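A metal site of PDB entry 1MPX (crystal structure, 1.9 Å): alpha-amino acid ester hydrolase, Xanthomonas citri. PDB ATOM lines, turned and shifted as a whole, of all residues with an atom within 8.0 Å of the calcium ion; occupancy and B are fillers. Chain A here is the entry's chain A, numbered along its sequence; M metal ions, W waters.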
ATOM      1  N   LEU A 273       7.506  19.807  21.511  1.00  0.00           N
ATOM      2  CA  LEU A 273       8.566  18.816  21.295  1.00  0.00           C
ATOM      3  C   LEU A 273       8.922  18.782  19.813  1.00  0.00           C
ATOM      4  O   LEU A 273       8.137  18.287  19.000  1.00  0.00           O
ATOM      5  CB  LEU A 273       8.101  17.418  21.735  1.00  0.00           C
ATOM      6  CG  LEU A 273       8.068  17.105  23.230  1.00  0.00           C
ATOM      7  CD1 LEU A 273       6.992  17.923  23.944  1.00  0.00           C
ATOM      8  CD2 LEU A 273       7.844  15.611  23.443  1.00  0.00           C
ATOM      9  N   THR A 277      15.439  15.172  22.388  1.00  0.00           N
ATOM     10  CA  THR A 277      16.104  15.577  23.626  1.00  0.00           C
ATOM     11  C   THR A 277      16.283  14.429  24.585  1.00  0.00           C
ATOM     12  O   THR A 277      15.371  13.656  24.800  1.00  0.00           O
ATOM     13  CB  THR A 277      15.285  16.698  24.303  1.00  0.00           C
ATOM     14  OG1 THR A 277      15.186  17.832  23.421  1.00  0.00           O
ATOM     15  CG2 THR A 277      15.999  17.253  25.537  1.00  0.00           C
ATOM     16  N   TYR A 296      11.972  15.881  32.082  1.00  0.00           N
ATOM     17  CA  TYR A 296      11.591  14.747  31.257  1.00  0.00           C
ATOM     18  C   TYR A 296      10.097  14.475  31.418  1.00  0.00           C
ATOM     19  O   TYR A 296       9.406  14.276  30.451  1.00  0.00           O
ATOM     20  CB  TYR A 296      12.373  13.495  31.684  1.00  0.00           C
ATOM     21  CG  TYR A 296      11.787  12.202  31.132  1.00  0.00           C
ATOM     22  CD1 TYR A 296      12.055  11.793  29.823  1.00  0.00           C
ATOM     23  CD2 TYR A 296      10.983  11.388  31.910  1.00  0.00           C
ATOM     24  CE1 TYR A 296      11.522  10.618  29.310  1.00  0.00           C
ATOM     25  CE2 TYR A 296      10.447  10.194  31.409  1.00  0.00           C
ATOM     26  CZ  TYR A 296      10.728   9.824  30.113  1.00  0.00           C
ATOM     27  OH  TYR A 296      10.199   8.662  29.604  1.00  0.00           O
ATOM     28  N   MET A 299       7.560  16.770  29.601  1.00  0.00           N
ATOM     29  CA  MET A 299       7.410  16.630  28.143  1.00  0.00           C
ATOM     30  C   MET A 299       7.006  15.236  27.639  1.00  0.00           C
ATOM     31  O   MET A 299       6.486  15.113  26.533  1.00  0.00           O
ATOM     32  CB  MET A 299       8.738  17.010  27.460  1.00  0.00           C
ATOM     33  CG  MET A 299       9.261  18.374  27.842  1.00  0.00           C
ATOM     34  SD  MET A 299      10.918  18.846  26.867  1.00  0.00           S
ATOM     35  CE  MET A 299      10.147  20.080  25.544  1.00  0.00           C
ATOM     36  N   GLU A 300       7.225  14.190  28.445  1.00  0.00           N
ATOM     37  CA  GLU A 300       6.960  12.807  28.006  1.00  0.00           C
ATOM     38  C   GLU A 300       5.503  12.490  27.576  1.00  0.00           C
ATOM     39  O   GLU A 300       5.316  11.746  26.613  1.00  0.00           O
ATOM     40  CB  GLU A 300       7.430  11.790  29.056  1.00  0.00           C
ATOM     41  CG  GLU A 300       7.362  10.319  28.612  1.00  0.00           C
ATOM     42  CD  GLU A 300       8.235   9.985  27.391  1.00  0.00           C
ATOM     43  OE1 GLU A 300       9.188  10.728  27.089  1.00  0.00           O
ATOM     44  OE2 GLU A 300       7.971   8.962  26.724  1.00  0.00           O
ATOM     45  N   PRO A 301       4.494  13.016  28.279  1.00  0.00           N
ATOM     46  CA  PRO A 301       3.088  12.760  27.872  1.00  0.00           C
ATOM     47  C   PRO A 301       2.780  13.214  26.411  1.00  0.00           C
ATOM     48  O   PRO A 301       1.861  12.678  25.801  1.00  0.00           O
ATOM     49  CB  PRO A 301       2.275  13.573  28.896  1.00  0.00           C
ATOM     50  CG  PRO A 301       3.170  13.695  30.074  1.00  0.00           C
ATOM     51  CD  PRO A 301       4.561  13.843  29.504  1.00  0.00           C
ATOM     52  N   ARG A 302       3.558  14.176  25.888  1.00  0.00           N
ATOM     53  CA  ARG A 302       3.367  14.671  24.514  1.00  0.00           C
ATOM     54  C   ARG A 302       4.386  14.056  23.513  1.00  0.00           C
ATOM     55  O   ARG A 302       4.467  14.494  22.360  1.00  0.00           O
ATOM     56  CB  ARG A 302       3.462  16.188  24.498  1.00  0.00           C
ATOM     57  CG  ARG A 302       2.363  16.876  25.270  1.00  0.00           C
ATOM     58  CD  ARG A 302       2.590  18.344  25.478  1.00  0.00           C
ATOM     59  NE  ARG A 302       3.777  18.583  26.328  1.00  0.00           N
ATOM     60  CZ  ARG A 302       4.666  19.564  26.123  1.00  0.00           C
ATOM     61  NH1 ARG A 302       4.533  20.406  25.119  1.00  0.00           N
ATOM     62  NH2 ARG A 302       5.690  19.692  26.953  1.00  0.00           N
ATOM     63  N   ASP A 303       5.155  13.060  23.960  1.00  0.00           N
ATOM     64  CA  ASP A 303       6.111  12.349  23.118  1.00  0.00           C
ATOM     65  C   ASP A 303       5.342  11.187  22.474  1.00  0.00           C
ATOM     66  O   ASP A 303       5.515  10.022  22.828  1.00  0.00           O
ATOM     67  CB  ASP A 303       7.290  11.845  23.974  1.00  0.00           C
ATOM     68  CG  ASP A 303       8.417  11.268  23.146  1.00  0.00           C
ATOM     69  OD1 ASP A 303       8.431  11.467  21.910  1.00  0.00           O
ATOM     70  OD2 ASP A 303       9.343  10.582  23.655  1.00  0.00           O
ATOM     71  N   LYS A 304       4.489  11.538  21.500  1.00  0.00           N
ATOM     72  CA  LYS A 304       3.553  10.600  20.823  1.00  0.00           C
ATOM     73  C   LYS A 304       4.154   9.296  20.294  1.00  0.00           C
ATOM     74  O   LYS A 304       3.612   8.221  20.527  1.00  0.00           O
ATOM     75  CB  LYS A 304       2.810  11.326  19.699  1.00  0.00           C
ATOM     76  CG  LYS A 304       1.828  12.421  20.176  1.00  0.00           C
ATOM     77  CD  LYS A 304       1.177  13.180  19.001  1.00  0.00           C
ATOM     78  CE  LYS A 304       1.902  14.499  18.700  1.00  0.00           C
ATOM     79  NZ  LYS A 304       1.162  15.317  17.691  1.00  0.00           N
ATOM     80  N   ARG A 305       5.266   9.396  19.564  1.00  0.00           N
ATOM     81  CA  ARG A 305       5.920   8.217  18.963  1.00  0.00           C
ATOM     82  C   ARG A 305       7.066   7.671  19.813  1.00  0.00           C
ATOM     83  O   ARG A 305       7.715   6.692  19.434  1.00  0.00           O
ATOM     84  CB  ARG A 305       6.438   8.564  17.562  1.00  0.00           C
ATOM     85  CG  ARG A 305       5.363   9.159  16.615  1.00  0.00           C
ATOM     86  CD  ARG A 305       4.219   8.204  16.280  1.00  0.00           C
ATOM     87  NE  ARG A 305       4.670   7.023  15.538  1.00  0.00           N
ATOM     88  CZ  ARG A 305       4.879   6.983  14.193  1.00  0.00           C
ATOM     89  NH1 ARG A 305       4.681   8.068  13.437  1.00  0.00           N
ATOM     90  NH2 ARG A 305       5.288   5.856  13.634  1.00  0.00           N
ATOM     91  N   ASN A 306       7.311   8.303  20.956  1.00  0.00           N
ATOM     92  CA  ASN A 306       8.393   7.904  21.872  1.00  0.00           C
ATOM     93  C   ASN A 306       9.794   8.001  21.213  1.00  0.00           C
ATOM     94  O   ASN A 306      10.667   7.168  21.472  1.00  0.00           O
ATOM     95  CB  ASN A 306       8.136   6.483  22.430  1.00  0.00           C
ATOM     96  CG  ASN A 306       8.688   6.297  23.855  1.00  0.00           C
ATOM     97  OD1 ASN A 306       9.166   7.250  24.477  1.00  0.00           O
ATOM     98  ND2 ASN A 306       8.624   5.086  24.367  1.00  0.00           N
ATOM     99  N   THR A 307      10.002   9.029  20.390  1.00  0.00           N
ATOM    100  CA  THR A 307      11.301   9.234  19.718  1.00  0.00           C
ATOM    101  C   THR A 307      11.840  10.671  19.851  1.00  0.00           C
ATOM    102  O   THR A 307      12.812  11.017  19.199  1.00  0.00           O
ATOM    103  CB  THR A 307      11.180   8.892  18.227  1.00  0.00           C
ATOM    104  OG1 THR A 307      10.089   9.611  17.642  1.00  0.00           O
ATOM    105  CG2 THR A 307      10.824   7.412  18.020  1.00  0.00           C
ATOM    106  N   LEU A 308      11.221  11.491  20.688  1.00  0.00           N
ATOM    107  CA  LEU A 308      11.652  12.896  20.856  1.00  0.00           C
ATOM    108  C   LEU A 308      12.077  13.271  22.279  1.00  0.00           C
ATOM    109  O   LEU A 308      12.700  14.301  22.485  1.00  0.00           O
ATOM    110  CB  LEU A 308      10.522  13.855  20.432  1.00  0.00           C
ATOM    111  CG  LEU A 308      10.334  14.087  18.931  1.00  0.00           C
ATOM    112  CD1 LEU A 308       9.055  14.913  18.695  1.00  0.00           C
ATOM    113  CD2 LEU A 308      11.548  14.781  18.311  1.00  0.00           C
ATOM    114  N   ASN A 309      11.758  12.422  23.262  1.00  0.00           N
ATOM    115  CA  ASN A 309      12.033  12.723  24.677  1.00  0.00           C
ATOM    116  C   ASN A 309      12.581  11.489  25.394  1.00  0.00           C
ATOM    117  O   ASN A 309      11.881  10.508  25.574  1.00  0.00           O
ATOM    118  CB  ASN A 309      10.737  13.217  25.340  1.00  0.00           C
ATOM    119  CG  ASN A 309      10.975  13.906  26.643  1.00  0.00           C
ATOM    120  OD1 ASN A 309      11.664  14.909  26.705  1.00  0.00           O
ATOM    121  ND2 ASN A 309      10.392  13.361  27.725  1.00  0.00           N
ATOM    122  N   TYR A 310      13.837  11.560  25.820  1.00  0.00           N
ATOM    123  CA  TYR A 310      14.522  10.433  26.435  1.00  0.00           C
ATOM    124  C   TYR A 310      14.983  10.723  27.863  1.00  0.00           C
ATOM    125  O   TYR A 310      15.114  11.882  28.264  1.00  0.00           O
ATOM    126  CB  TYR A 310      15.728  10.029  25.576  1.00  0.00           C
ATOM    127  CG  TYR A 310      15.338   9.497  24.212  1.00  0.00           C
ATOM    128  CD1 TYR A 310      15.015  10.362  23.163  1.00  0.00           C
ATOM    129  CD2 TYR A 310      15.271   8.141  23.981  1.00  0.00           C
ATOM    130  CE1 TYR A 310      14.648   9.879  21.933  1.00  0.00           C
ATOM    131  CE2 TYR A 310      14.909   7.638  22.756  1.00  0.00           C
ATOM    132  CZ  TYR A 310      14.596   8.501  21.730  1.00  0.00           C
ATOM    133  OH  TYR A 310      14.227   7.999  20.511  1.00  0.00           O
ATOM    134  N   LEU A 311      15.222   9.649  28.618  1.00  0.00           N
ATOM    135  CA  LEU A 311      15.683   9.756  29.987  1.00  0.00           C
ATOM    136  C   LEU A 311      16.859   8.845  30.204  1.00  0.00           C
ATOM    137  O   LEU A 311      16.856   7.720  29.761  1.00  0.00           O
ATOM    138  CB  LEU A 311      14.564   9.353  30.969  1.00  0.00           C
ATOM    139  CG  LEU A 311      14.943   9.376  32.481  1.00  0.00           C
ATOM    140  CD1 LEU A 311      15.273  10.824  32.941  1.00  0.00           C
ATOM    141  CD2 LEU A 311      13.830   8.783  33.326  1.00  0.00           C
ATOM    142  N   PRO A 364      17.231   3.450  23.629  1.00  0.00           N
ATOM    143  CA  PRO A 364      16.201   3.062  24.573  1.00  0.00           C
ATOM    144  C   PRO A 364      15.493   4.319  25.068  1.00  0.00           C
ATOM    145  O   PRO A 364      16.190   5.256  25.428  1.00  0.00           O
ATOM    146  CB  PRO A 364      16.986   2.404  25.712  1.00  0.00           C
ATOM    147  CG  PRO A 364      18.351   2.964  25.612  1.00  0.00           C
ATOM    148  CD  PRO A 364      18.584   3.303  24.187  1.00  0.00           C
ATOM    149  N   PRO A 365      14.152   4.360  25.036  1.00  0.00           N
ATOM    150  CA  PRO A 365      13.417   5.527  25.544  1.00  0.00           C
ATOM    151  C   PRO A 365      13.878   5.928  26.947  1.00  0.00           C
ATOM    152  O   PRO A 365      13.904   7.116  27.274  1.00  0.00           O
ATOM    153  CB  PRO A 365      11.975   5.051  25.543  1.00  0.00           C
ATOM    154  CG  PRO A 365      11.922   4.069  24.412  1.00  0.00           C
ATOM    155  CD  PRO A 365      13.244   3.331  24.483  1.00  0.00           C
ATOM    156  N   VAL A 366      14.245   4.933  27.758  1.00  0.00           N
ATOM    157  CA  VAL A 366      14.732   5.138  29.112  1.00  0.00           C
ATOM    158  C   VAL A 366      15.961   4.222  29.338  1.00  0.00           C
ATOM    159  O   VAL A 366      15.904   3.021  29.079  1.00  0.00           O
ATOM    160  CB  VAL A 366      13.644   4.828  30.182  1.00  0.00           C
ATOM    161  CG1 VAL A 366      14.224   4.966  31.597  1.00  0.00           C
ATOM    162  CG2 VAL A 366      12.438   5.751  30.006  1.00  0.00           C
ATOM    163  N   LEU A 379      14.267   0.525  29.057  1.00  0.00           N
ATOM    164  CA  LEU A 379      12.805   0.554  29.200  1.00  0.00           C
ATOM    165  C   LEU A 379      12.130   1.529  28.244  1.00  0.00           C
ATOM    166  O   LEU A 379      12.768   2.402  27.681  1.00  0.00           O
ATOM    167  CB  LEU A 379      12.433   0.936  30.644  1.00  0.00           C
ATOM    168  CG  LEU A 379      13.135   0.139  31.741  1.00  0.00           C
ATOM    169  CD1 LEU A 379      13.038   0.856  33.083  1.00  0.00           C
ATOM    170  CD2 LEU A 379      12.551  -1.253  31.844  1.00  0.00           C
ATOM    171  N   LYS A 380      10.821   1.365  28.071  1.00  0.00           N
ATOM    172  CA  LYS A 380      10.026   2.220  27.191  1.00  0.00           C
ATOM    173  C   LYS A 380       9.398   3.381  27.956  1.00  0.00           C
ATOM    174  O   LYS A 380       8.955   4.362  27.351  1.00  0.00           O
ATOM    175  CB  LYS A 380       8.917   1.414  26.503  1.00  0.00           C
ATOM    176  CG  LYS A 380       9.419   0.517  25.383  1.00  0.00           C
ATOM    177  CD  LYS A 380       8.313  -0.411  24.891  1.00  0.00           C
ATOM    178  CE  LYS A 380       8.832  -1.367  23.814  1.00  0.00           C
ATOM    179  NZ  LYS A 380       7.734  -2.248  23.289  1.00  0.00           N
ATOM    180  N   ALA A 381       9.351   3.270  29.288  1.00  0.00           N
ATOM    181  CA  ALA A 381       8.762   4.290  30.130  1.00  0.00           C
ATOM    182  C   ALA A 381       9.358   4.336  31.545  1.00  0.00           C
ATOM    183  O   ALA A 381      10.008   3.375  32.004  1.00  0.00           O
ATOM    184  CB  ALA A 381       7.226   4.083  30.210  1.00  0.00           C
ATOM    185  N   TRP A 382       9.110   5.449  32.219  1.00  0.00           N
ATOM    186  CA  TRP A 382       9.548   5.678  33.596  1.00  0.00           C
ATOM    187  C   TRP A 382       8.654   6.795  34.201  1.00  0.00           C
ATOM    188  O   TRP A 382       8.362   7.776  33.518  1.00  0.00           O
ATOM    189  CB  TRP A 382      11.027   6.102  33.646  1.00  0.00           C
ATOM    190  CG  TRP A 382      11.522   6.165  35.020  1.00  0.00           C
ATOM    191  CD1 TRP A 382      11.501   7.246  35.843  1.00  0.00           C
ATOM    192  CD2 TRP A 382      12.041   5.082  35.781  1.00  0.00           C
ATOM    193  NE1 TRP A 382      11.997   6.903  37.071  1.00  0.00           N
ATOM    194  CE2 TRP A 382      12.327   5.576  37.058  1.00  0.00           C
ATOM    195  CE3 TRP A 382      12.284   3.736  35.517  1.00  0.00           C
ATOM    196  CZ2 TRP A 382      12.864   4.779  38.065  1.00  0.00           C
ATOM    197  CZ3 TRP A 382      12.819   2.948  36.522  1.00  0.00           C
ATOM    198  CH2 TRP A 382      13.098   3.464  37.764  1.00  0.00           C
HETATM  199 CA    CA M   1      10.104   9.106  25.354  1.00  0.00          CA
HETATM  200  O   HOH W   1      11.769   8.242  23.971  1.00  0.00           O
HETATM  201  O   HOH W   2      11.202   7.960  27.178  1.00  0.00           O
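The side-chain amide nitrogen (ND2) of Asn 306 is in hydrogen-bond range of the backbone carbonyl oxygen (O) of Lys 380 (3.1 Å).
ND2 of Asn 309 is in hydrogen-bond range of O of Tyr 296, 3.0 Å away.
OD1 of Asp 303 is in hydrogen-bond range of N of Thr 307 (3.3 Å).
OD1 of Asp 303 is in hydrogen-bond range of N of Leu 308.
OH of Tyr 296 sits close to OE1 of Glu 300.
Within 4 Å of the calcium ion: Glu 300, Asp 303, Asn 306 and Asn 309.
OD1 of Asn 306 is bound to the calcium ion (2.3 Å).
O of Asn 309 is bound to the calcium ion (2.3 Å).
The calcium ion is bound by water W1, 2.3 Å away.
The calcium ion is bound by the side-chain carboxylate (OD2) of Asp 303, at 2.4 Å.
Water W2 binds the calcium ion (2.4 Å).
The calcium ion is bound by OE2 of Glu 300 (2.5 Å).
OE1 of Glu 300 is bound to the calcium ion, 2.5 Å away.
The calcium ion has seven donor atoms within binding distance.
Water W2 bridges the side-chain hydroxyl of Tyr 296 (2.7 Å) and the backbone carbonyl oxygen of Pro 365 (2.8 Å).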
